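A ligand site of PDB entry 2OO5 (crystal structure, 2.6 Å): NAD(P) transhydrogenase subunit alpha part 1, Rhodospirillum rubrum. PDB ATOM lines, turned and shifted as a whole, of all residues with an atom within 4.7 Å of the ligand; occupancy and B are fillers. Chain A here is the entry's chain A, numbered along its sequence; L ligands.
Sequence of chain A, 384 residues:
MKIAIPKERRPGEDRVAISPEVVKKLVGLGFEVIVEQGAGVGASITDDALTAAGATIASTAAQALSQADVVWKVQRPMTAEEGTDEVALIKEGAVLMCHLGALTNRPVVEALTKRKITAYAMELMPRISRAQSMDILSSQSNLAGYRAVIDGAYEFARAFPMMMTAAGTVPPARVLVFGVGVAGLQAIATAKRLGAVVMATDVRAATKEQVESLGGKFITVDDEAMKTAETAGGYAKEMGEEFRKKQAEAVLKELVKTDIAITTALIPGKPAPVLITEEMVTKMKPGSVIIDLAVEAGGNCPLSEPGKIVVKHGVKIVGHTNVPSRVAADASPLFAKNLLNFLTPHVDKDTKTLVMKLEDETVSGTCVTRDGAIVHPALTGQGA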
ATOM      1  N   PRO A 126     -15.529 -16.689   8.780  1.00  0.00           N
ATOM      2  CA  PRO A 126     -16.888 -16.554   8.259  1.00  0.00           C
ATOM      3  C   PRO A 126     -17.179 -17.482   7.078  1.00  0.00           C
ATOM      4  O   PRO A 126     -16.279 -17.787   6.296  1.00  0.00           O
ATOM      5  CB  PRO A 126     -16.971 -15.087   7.813  1.00  0.00           C
ATOM      6  CG  PRO A 126     -15.846 -14.399   8.494  1.00  0.00           C
ATOM      7  CD  PRO A 126     -14.772 -15.428   8.621  1.00  0.00           C
ATOM      8  N   ARG A 127     -18.437 -17.913   6.962  1.00  0.00           N
ATOM      9  CA  ARG A 127     -18.857 -18.850   5.931  1.00  0.00           C
ATOM     10  C   ARG A 127     -19.123 -18.075   4.640  1.00  0.00           C
ATOM     11  O   ARG A 127     -20.282 -17.792   4.298  1.00  0.00           O
ATOM     12  CB  ARG A 127     -20.125 -19.616   6.358  1.00  0.00           C
ATOM     13  CG  ARG A 127     -20.099 -20.258   7.746  1.00  0.00           C
ATOM     14  CD  ARG A 127     -18.998 -21.286   7.913  1.00  0.00           C
ATOM     15  NE  ARG A 127     -19.098 -21.972   9.196  1.00  0.00           N
ATOM     16  CZ  ARG A 127     -19.952 -22.954   9.506  1.00  0.00           C
ATOM     17  NH1 ARG A 127     -20.840 -23.426   8.627  1.00  0.00           N
ATOM     18  NH2 ARG A 127     -19.926 -23.483  10.732  1.00  0.00           N
ATOM     19  N   ILE A 128     -18.058 -17.705   3.939  1.00  0.00           N
ATOM     20  CA  ILE A 128     -18.167 -16.974   2.672  1.00  0.00           C
ATOM     21  C   ILE A 128     -17.240 -17.590   1.630  1.00  0.00           C
ATOM     22  O   ILE A 128     -16.124 -17.993   1.966  1.00  0.00           O
ATOM     23  CB  ILE A 128     -17.883 -15.449   2.818  1.00  0.00           C
ATOM     24  CG1 ILE A 128     -16.551 -15.183   3.537  1.00  0.00           C
ATOM     25  CG2 ILE A 128     -19.018 -14.777   3.584  1.00  0.00           C
ATOM     26  CD1 ILE A 128     -15.994 -13.789   3.294  1.00  0.00           C
ATOM     27  N   SER A 129     -17.713 -17.664   0.386  1.00  0.00           N
ATOM     28  CA  SER A 129     -17.018 -18.323  -0.740  1.00  0.00           C
ATOM     29  C   SER A 129     -15.495 -18.179  -0.745  1.00  0.00           C
ATOM     30  O   SER A 129     -14.762 -19.161  -0.785  1.00  0.00           O
ATOM     31  CB  SER A 129     -17.564 -17.793  -2.064  1.00  0.00           C
ATOM     32  OG  SER A 129     -18.904 -18.213  -2.274  1.00  0.00           O
ATOM     33  N   ALA A 131     -13.443 -17.319   1.575  1.00  0.00           N
ATOM     34  CA  ALA A 131     -12.779 -17.842   2.771  1.00  0.00           C
ATOM     35  C   ALA A 131     -12.799 -19.382   2.876  1.00  0.00           C
ATOM     36  O   ALA A 131     -12.455 -19.925   3.924  1.00  0.00           O
ATOM     37  CB  ALA A 131     -13.384 -17.217   4.025  1.00  0.00           C
ATOM     38  N   GLN A 132     -13.189 -20.077   1.811  1.00  0.00           N
ATOM     39  CA  GLN A 132     -13.170 -21.548   1.793  1.00  0.00           C
ATOM     40  C   GLN A 132     -11.763 -22.123   1.888  1.00  0.00           C
ATOM     41  O   GLN A 132     -11.570 -23.166   2.522  1.00  0.00           O
ATOM     42  CB  GLN A 132     -13.891 -22.132   0.561  1.00  0.00           C
ATOM     43  CG  GLN A 132     -15.357 -22.386   0.837  1.00  0.00           C
ATOM     44  CD  GLN A 132     -16.151 -22.686  -0.423  1.00  0.00           C
ATOM     45  OE1 GLN A 132     -15.849 -23.613  -1.170  1.00  0.00           O
ATOM     46  NE2 GLN A 132     -17.204 -21.902  -0.646  1.00  0.00           N
ATOM     47  N   ASP A 135     -10.401 -21.967   5.730  1.00  0.00           N
ATOM     48  CA  ASP A 135     -11.270 -22.511   6.783  1.00  0.00           C
ATOM     49  C   ASP A 135     -10.767 -23.844   7.350  1.00  0.00           C
ATOM     50  O   ASP A 135     -10.818 -24.863   6.676  1.00  0.00           O
ATOM     51  CB  ASP A 135     -12.703 -22.673   6.271  1.00  0.00           C
ATOM     52  CG  ASP A 135     -13.690 -22.968   7.378  1.00  0.00           C
ATOM     53  OD1 ASP A 135     -13.555 -22.401   8.488  1.00  0.00           O
ATOM     54  OD2 ASP A 135     -14.609 -23.772   7.149  1.00  0.00           O
ATOM     55  N   SER A 138     -13.323 -26.898   7.919  1.00  0.00           N
ATOM     56  CA  SER A 138     -13.709 -27.550   6.691  1.00  0.00           C
ATOM     57  C   SER A 138     -12.633 -28.504   6.174  1.00  0.00           C
ATOM     58  O   SER A 138     -12.943 -29.645   5.807  1.00  0.00           O
ATOM     59  CB  SER A 138     -14.024 -26.470   5.640  1.00  0.00           C
ATOM     60  OG  SER A 138     -14.264 -27.033   4.375  1.00  0.00           O
ATOM     61  N   SER A 141     -12.397 -31.460   9.003  1.00  0.00           N
ATOM     62  CA  SER A 141     -13.583 -32.334   9.054  1.00  0.00           C
ATOM     63  C   SER A 141     -13.721 -33.229   7.813  1.00  0.00           C
ATOM     64  O   SER A 141     -14.295 -34.321   7.912  1.00  0.00           O
ATOM     65  CB  SER A 141     -14.869 -31.526   9.237  1.00  0.00           C
ATOM     66  OG  SER A 141     -15.204 -30.818   8.063  1.00  0.00           O
ATOM     67  N   GLY A 179     -26.074 -36.488   8.881  1.00  0.00           N
ATOM     68  CA  GLY A 179     -25.470 -35.177   8.655  1.00  0.00           C
ATOM     69  C   GLY A 179     -24.521 -35.244   7.476  1.00  0.00           C
ATOM     70  O   GLY A 179     -23.453 -35.856   7.558  1.00  0.00           O
ATOM     71  N   VAL A 180     -24.926 -34.618   6.362  1.00  0.00           N
ATOM     72  CA  VAL A 180     -24.144 -34.618   5.124  1.00  0.00           C
ATOM     73  C   VAL A 180     -23.520 -33.236   4.926  1.00  0.00           C
ATOM     74  O   VAL A 180     -23.857 -32.491   4.008  1.00  0.00           O
ATOM     75  CB  VAL A 180     -25.014 -35.042   3.897  1.00  0.00           C
ATOM     76  CG1 VAL A 180     -24.138 -35.289   2.671  1.00  0.00           C
ATOM     77  CG2 VAL A 180     -25.813 -36.303   4.222  1.00  0.00           C
ATOM     78  N   GLY A 181     -22.590 -32.906   5.822  1.00  0.00           N
ATOM     79  CA  GLY A 181     -21.760 -31.715   5.686  1.00  0.00           C
ATOM     80  C   GLY A 181     -20.511 -32.058   4.908  1.00  0.00           C
ATOM     81  O   GLY A 181     -20.540 -32.932   4.036  1.00  0.00           O
ATOM     82  N   VAL A 182     -19.410 -31.383   5.222  1.00  0.00           N
ATOM     83  CA  VAL A 182     -18.139 -31.650   4.578  1.00  0.00           C
ATOM     84  C   VAL A 182     -17.621 -33.042   4.980  1.00  0.00           C
ATOM     85  O   VAL A 182     -17.093 -33.780   4.142  1.00  0.00           O
ATOM     86  CB  VAL A 182     -17.096 -30.552   4.908  1.00  0.00           C
ATOM     87  CG1 VAL A 182     -15.727 -30.899   4.320  1.00  0.00           C
ATOM     88  CG2 VAL A 182     -17.574 -29.184   4.382  1.00  0.00           C
ATOM     89  N   ALA A 183     -17.774 -33.374   6.263  1.00  0.00           N
ATOM     90  CA  ALA A 183     -17.400 -34.683   6.797  1.00  0.00           C
ATOM     91  C   ALA A 183     -18.290 -35.804   6.258  1.00  0.00           C
ATOM     92  O   ALA A 183     -17.792 -36.860   5.872  1.00  0.00           O
ATOM     93  CB  ALA A 183     -17.462 -34.657   8.319  1.00  0.00           C
ATOM     94  N   THR A 201     -28.882 -38.853   5.427  1.00  0.00           N
ATOM     95  CA  THR A 201     -29.959 -37.924   5.760  1.00  0.00           C
ATOM     96  C   THR A 201     -29.405 -36.596   6.289  1.00  0.00           C
ATOM     97  O   THR A 201     -28.278 -36.537   6.800  1.00  0.00           O
ATOM     98  CB  THR A 201     -30.959 -38.549   6.772  1.00  0.00           C
ATOM     99  OG1 THR A 201     -32.109 -37.705   6.897  1.00  0.00           O
ATOM    100  CG2 THR A 201     -30.319 -38.770   8.143  1.00  0.00           C
ATOM    101  N   ASP A 202     -30.195 -35.529   6.143  1.00  0.00           N
ATOM    102  CA  ASP A 202     -29.787 -34.164   6.498  1.00  0.00           C
ATOM    103  C   ASP A 202     -31.029 -33.268   6.495  1.00  0.00           C
ATOM    104  O   ASP A 202     -32.023 -33.585   5.837  1.00  0.00           O
ATOM    105  CB  ASP A 202     -28.763 -33.630   5.483  1.00  0.00           C
ATOM    106  CG  ASP A 202     -27.978 -32.419   5.981  1.00  0.00           C
ATOM    107  OD1 ASP A 202     -28.586 -31.379   6.304  1.00  0.00           O
ATOM    108  OD2 ASP A 202     -26.735 -32.498   6.022  1.00  0.00           O
ATOM    109  N   VAL A 203     -30.958 -32.161   7.225  1.00  0.00           N
ATOM    110  CA  VAL A 203     -32.043 -31.170   7.240  1.00  0.00           C
ATOM    111  C   VAL A 203     -32.052 -30.245   6.011  1.00  0.00           C
ATOM    112  O   VAL A 203     -33.122 -29.825   5.579  1.00  0.00           O
ATOM    113  CB  VAL A 203     -32.062 -30.302   8.549  1.00  0.00           C
ATOM    114  CG1 VAL A 203     -32.188 -31.193   9.774  1.00  0.00           C
ATOM    115  CG2 VAL A 203     -30.832 -29.391   8.658  1.00  0.00           C
ATOM    116  N   ARG A 204     -30.882 -29.926   5.458  1.00  0.00           N
ATOM    117  CA  ARG A 204     -30.777 -29.004   4.320  1.00  0.00           C
ATOM    118  C   ARG A 204     -31.170 -29.684   3.014  1.00  0.00           C
ATOM    119  O   ARG A 204     -30.698 -30.778   2.721  1.00  0.00           O
ATOM    120  CB  ARG A 204     -29.352 -28.444   4.220  1.00  0.00           C
ATOM    121  CG  ARG A 204     -28.910 -27.659   5.439  1.00  0.00           C
ATOM    122  CD  ARG A 204     -27.579 -26.949   5.248  1.00  0.00           C
ATOM    123  NE  ARG A 204     -26.454 -27.851   4.976  1.00  0.00           N
ATOM    124  CZ  ARG A 204     -25.942 -28.149   3.775  1.00  0.00           C
ATOM    125  NH1 ARG A 204     -26.409 -27.621   2.643  1.00  0.00           N
ATOM    126  NH2 ARG A 204     -24.912 -28.987   3.701  1.00  0.00           N
ATOM    127  N   GLY A 234     -25.163 -20.998   5.458  1.00  0.00           N
ATOM    128  CA  GLY A 234     -25.229 -22.292   4.782  1.00  0.00           C
ATOM    129  C   GLY A 234     -25.105 -23.479   5.725  1.00  0.00           C
ATOM    130  O   GLY A 234     -24.507 -24.480   5.368  1.00  0.00           O
ATOM    131  N   TYR A 235     -25.700 -23.363   6.916  1.00  0.00           N
ATOM    132  CA  TYR A 235     -25.685 -24.434   7.916  1.00  0.00           C
ATOM    133  C   TYR A 235     -27.073 -24.617   8.521  1.00  0.00           C
ATOM    134  O   TYR A 235     -27.995 -23.838   8.239  1.00  0.00           O
ATOM    135  CB  TYR A 235     -24.628 -24.131   9.009  1.00  0.00           C
ATOM    136  CG  TYR A 235     -24.775 -22.787   9.693  1.00  0.00           C
ATOM    137  CD1 TYR A 235     -25.514 -22.672  10.873  1.00  0.00           C
ATOM    138  CD2 TYR A 235     -24.157 -21.650   9.195  1.00  0.00           C
ATOM    139  CE1 TYR A 235     -25.650 -21.438  11.520  1.00  0.00           C
ATOM    140  CE2 TYR A 235     -24.289 -20.421   9.834  1.00  0.00           C
ATOM    141  CZ  TYR A 235     -25.040 -20.324  10.993  1.00  0.00           C
ATOM    142  OH  TYR A 235     -25.170 -19.111  11.632  1.00  0.00           O
ATOM    143  N   ALA A 236     -27.243 -25.656   9.329  1.00  0.00           N
ATOM    144  CA  ALA A 236     -28.555 -26.040   9.877  1.00  0.00           C
ATOM    145  C   ALA A 236     -29.012 -25.133  11.024  1.00  0.00           C
ATOM    146  O   ALA A 236     -28.211 -24.427  11.621  1.00  0.00           O
ATOM    147  CB  ALA A 236     -28.517 -27.482  10.347  1.00  0.00           C
ATOM    148  N   GLN A 247     -38.367 -37.631  11.931  1.00  0.00           N
ATOM    149  CA  GLN A 247     -37.045 -38.054  11.466  1.00  0.00           C
ATOM    150  C   GLN A 247     -36.652 -39.430  11.991  1.00  0.00           C
ATOM    151  O   GLN A 247     -36.160 -40.259  11.225  1.00  0.00           O
ATOM    152  CB  GLN A 247     -35.985 -37.031  11.886  1.00  0.00           C
ATOM    153  CG  GLN A 247     -34.586 -37.276  11.283  1.00  0.00           C
ATOM    154  CD  GLN A 247     -33.565 -36.251  11.734  1.00  0.00           C
ATOM    155  OE1 GLN A 247     -32.888 -35.636  10.914  1.00  0.00           O
ATOM    156  NE2 GLN A 247     -33.447 -36.066  13.040  1.00  0.00           N
ATOM    157  N   THR A 264     -22.391 -37.102  12.099  1.00  0.00           N
ATOM    158  CA  THR A 264     -21.527 -35.919  11.960  1.00  0.00           C
ATOM    159  C   THR A 264     -22.252 -34.580  12.181  1.00  0.00           C
ATOM    160  O   THR A 264     -21.672 -33.520  11.933  1.00  0.00           O
ATOM    161  CB  THR A 264     -20.903 -35.855  10.536  1.00  0.00           C
ATOM    162  OG1 THR A 264     -21.787 -35.178   9.633  1.00  0.00           O
ATOM    163  CG2 THR A 264     -20.601 -37.262   9.996  1.00  0.00           C
ATOM    164  N   ALA A 265     -23.495 -34.632  12.678  1.00  0.00           N
ATOM    165  CA  ALA A 265     -24.372 -33.454  12.688  1.00  0.00           C
ATOM    166  C   ALA A 265     -23.997 -32.447  13.765  1.00  0.00           C
ATOM    167  O   ALA A 265     -23.814 -32.810  14.932  1.00  0.00           O
ATOM    168  CB  ALA A 265     -25.818 -33.878  12.840  1.00  0.00           C
ATOM    169  N   LEU A 266     -23.917 -31.169  13.355  1.00  0.00           N
ATOM    170  CA  LEU A 266     -23.513 -30.057  14.211  1.00  0.00           C
ATOM    171  C   LEU A 266     -24.441 -28.850  13.984  1.00  0.00           C
ATOM    172  O   LEU A 266     -24.840 -28.571  12.852  1.00  0.00           O
ATOM    173  CB  LEU A 266     -22.059 -29.652  13.902  1.00  0.00           C
ATOM    174  CG  LEU A 266     -20.932 -30.007  14.884  1.00  0.00           C
ATOM    175  CD1 LEU A 266     -20.938 -31.482  15.272  1.00  0.00           C
ATOM    176  CD2 LEU A 266     -19.588 -29.602  14.285  1.00  0.00           C
ATOM    177  N   ILE A 267     -24.761 -28.138  15.063  1.00  0.00           N
ATOM    178  CA  ILE A 267     -25.535 -26.886  14.996  1.00  0.00           C
ATOM    179  C   ILE A 267     -24.655 -25.790  15.642  1.00  0.00           C
ATOM    180  O   ILE A 267     -24.600 -25.708  16.865  1.00  0.00           O
ATOM    181  CB  ILE A 267     -26.907 -27.017  15.720  1.00  0.00           C
ATOM    182  CG1 ILE A 267     -27.760 -28.115  15.051  1.00  0.00           C
ATOM    183  CG2 ILE A 267     -27.675 -25.677  15.675  1.00  0.00           C
ATOM    184  CD1 ILE A 267     -28.979 -28.559  15.854  1.00  0.00           C
ATOM    185  N   PRO A 268     -23.944 -24.969  14.829  1.00  0.00           N
ATOM    186  CA  PRO A 268     -22.953 -23.983  15.317  1.00  0.00           C
ATOM    187  C   PRO A 268     -23.393 -23.110  16.498  1.00  0.00           C
ATOM    188  O   PRO A 268     -24.404 -22.412  16.413  1.00  0.00           O
ATOM    189  CB  PRO A 268     -22.703 -23.116  14.083  1.00  0.00           C
ATOM    190  CG  PRO A 268     -22.906 -24.019  12.946  1.00  0.00           C
ATOM    191  CD  PRO A 268     -24.018 -24.939  13.353  1.00  0.00           C
ATOM    192  N   PRO A 273     -27.235 -32.015  18.013  1.00  0.00           N
ATOM    193  CA  PRO A 273     -28.562 -32.613  18.112  1.00  0.00           C
ATOM    194  C   PRO A 273     -28.531 -34.132  18.271  1.00  0.00           C
ATOM    195  O   PRO A 273     -27.783 -34.794  17.552  1.00  0.00           O
ATOM    196  CB  PRO A 273     -29.207 -32.231  16.772  1.00  0.00           C
ATOM    197  CG  PRO A 273     -28.077 -32.124  15.837  1.00  0.00           C
ATOM    198  CD  PRO A 273     -26.924 -31.598  16.635  1.00  0.00           C
ATOM    199  N   LEU A 275     -29.446 -37.477  17.446  1.00  0.00           N
ATOM    200  CA  LEU A 275     -30.042 -38.155  16.282  1.00  0.00           C
ATOM    201  C   LEU A 275     -30.270 -39.646  16.466  1.00  0.00           C
ATOM    202  O   LEU A 275     -31.133 -40.223  15.811  1.00  0.00           O
ATOM    203  CB  LEU A 275     -29.166 -37.926  15.040  1.00  0.00           C
ATOM    204  CG  LEU A 275     -28.723 -36.495  14.735  1.00  0.00           C
ATOM    205  CD1 LEU A 275     -28.065 -36.434  13.372  1.00  0.00           C
ATOM    206  CD2 LEU A 275     -29.863 -35.481  14.811  1.00  0.00           C
HETATM  207  O1  LIG L   1     -18.248 -21.388   2.033  1.00  0.00           O
HETATM  208  C1  LIG L   1     -17.762 -21.647   3.131  1.00  0.00           C
HETATM  209  N1  LIG L   1     -16.902 -20.825   3.719  1.00  0.00           N
HETATM  210  C2  LIG L   1     -18.106 -22.920   3.850  1.00  0.00           C
HETATM  211  C3  LIG L   1     -19.264 -23.623   3.511  1.00  0.00           C
HETATM  212  C4  LIG L   1     -17.165 -23.421   4.913  1.00  0.00           C
HETATM  213  C5  LIG L   1     -17.642 -24.669   5.514  1.00  0.00           C
HETATM  214  C6  LIG L   1     -18.813 -25.285   5.106  1.00  0.00           C
HETATM  215  N2  LIG L   1     -19.593 -24.765   4.131  1.00  0.00           N
HETATM  216  C7  LIG L   1     -20.836 -25.451   3.720  1.00  0.00           C
HETATM  217  O2  LIG L   1     -21.756 -25.577   4.810  1.00  0.00           O
HETATM  218  C8  LIG L   1     -20.609 -26.859   3.207  1.00  0.00           C
HETATM  219  O3  LIG L   1     -20.228 -26.847   1.834  1.00  0.00           O
HETATM  220  C9  LIG L   1     -21.960 -27.497   3.457  1.00  0.00           C
HETATM  221  O4  LIG L   1     -22.833 -27.261   2.350  1.00  0.00           O
HETATM  222  C10 LIG L   1     -22.496 -26.784   4.685  1.00  0.00           C
HETATM  223  C11 LIG L   1     -22.368 -27.566   5.986  1.00  0.00           C
HETATM  224  O5  LIG L   1     -20.993 -27.863   6.228  1.00  0.00           O
HETATM  225  P1  LIG L   1     -20.371 -28.133   7.692  1.00  0.00           P
HETATM  226  O6  LIG L   1     -19.494 -29.350   7.575  1.00  0.00           O
HETATM  227  O7  LIG L   1     -19.795 -26.831   8.198  1.00  0.00           O
HETATM  228  O8  LIG L   1     -21.659 -28.521   8.578  1.00  0.00           O
HETATM  229  P2  LIG L   1     -21.605 -28.781  10.166  1.00  0.00           P
HETATM  230  O9  LIG L   1     -22.130 -27.536  10.847  1.00  0.00           O
HETATM  231  O10 LIG L   1     -20.250 -29.320  10.570  1.00  0.00           O
HETATM  232  O11 LIG L   1     -22.723 -29.924  10.366  1.00  0.00           O
HETATM  233  C12 LIG L   1     -22.794 -31.070   9.528  1.00  0.00           C
HETATM  234  C13 LIG L   1     -24.161 -31.258   8.870  1.00  0.00           C
HETATM  235  C14 LIG L   1     -24.787 -30.017   8.232  1.00  0.00           C
HETATM  236  O12 LIG L   1     -24.804 -30.174   6.814  1.00  0.00           O
HETATM  237  C15 LIG L   1     -26.195 -29.934   8.798  1.00  0.00           C
HETATM  238  O13 LIG L   1     -27.165 -29.640   7.798  1.00  0.00           O
HETATM  239  C16 LIG L   1     -26.416 -31.310   9.415  1.00  0.00           C
HETATM  240  O14 LIG L   1     -25.116 -31.738   9.817  1.00  0.00           O
HETATM  241  N3  LIG L   1     -27.388 -31.343  10.545  1.00  0.00           N
HETATM  242  C17 LIG L   1     -28.367 -32.252  10.681  1.00  0.00           C
HETATM  243  N4  LIG L   1     -28.766 -33.302   9.918  1.00  0.00           N
HETATM  244  C18 LIG L   1     -29.804 -34.081  10.279  1.00  0.00           C
HETATM  245  N5  LIG L   1     -30.500 -33.850  11.414  1.00  0.00           N
HETATM  246  C19 LIG L   1     -30.176 -32.832  12.239  1.00  0.00           C
HETATM  247  N6  LIG L   1     -30.869 -32.590  13.367  1.00  0.00           N
HETATM  248  C20 LIG L   1     -29.033 -31.962  11.858  1.00  0.00           C
HETATM  249  N7  LIG L   1     -28.452 -30.893  12.425  1.00  0.00           N
HETATM  250  C21 LIG L   1     -27.444 -30.526  11.614  1.00  0.00           C
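OD1 of Asp 202 lies within hydrogen-bond range of O13 of the ligand.
NE2 of Gln 132 is in hydrogen-bond range of O1 of the ligand.
The guanidinium group (NH2) of Arg 204 sits at hydrogen-bond distance from an oxygen (O4) of the ligand (3.0 Å).
OE1 of Gln 247 lies close to N5 of the ligand, 3.0 Å away.
An oxygen (O6) of the ligand is in hydrogen-bond range of the backbone NH (N) of Val 182 (3.1 Å).
O of Ile 128 lies within hydrogen-bond range of N1 of the ligand (3.4 Å).
N of Leu 266 lies within hydrogen-bond range of O11 of the ligand, 3.5 Å away.
NH1 of Arg 127 is in salt-bridge range of O7 of the ligand.
OD1 of Asp 202 lies within hydrogen-bond range of N of Arg 204.
The side-chain carboxylate of Asp 202 lies within hydrogen-bond range of the backbone NH of Val 180 (2.8 Å).
N of Ser 138 lies close to OD2 of Asp 135 (3.5 Å).
The side-chain hydroxyl of Thr 264 sits at hydrogen-bond distance from the backbone carbonyl oxygen of Gly 179, at 2.7 Å.
The backbone NH (N) of Gly 179 sits at hydrogen-bond distance from the backbone carbonyl oxygen (O) of Thr 201 (3.0 Å).
An oxygen (O2) of the ligand lies close to the backbone carbonyl oxygen of Gly 234 (3.0 Å).
Residues that only touch the ligand: Asp 135, Gly 179, Val 180, Gly 181, Val 203, Ala 236, Thr 264, Ala 265, Ile 267, Pro 273 and Leu 275.
The nearest printed residue that does not touch the ligand is Pro 126 (4.03 Å).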
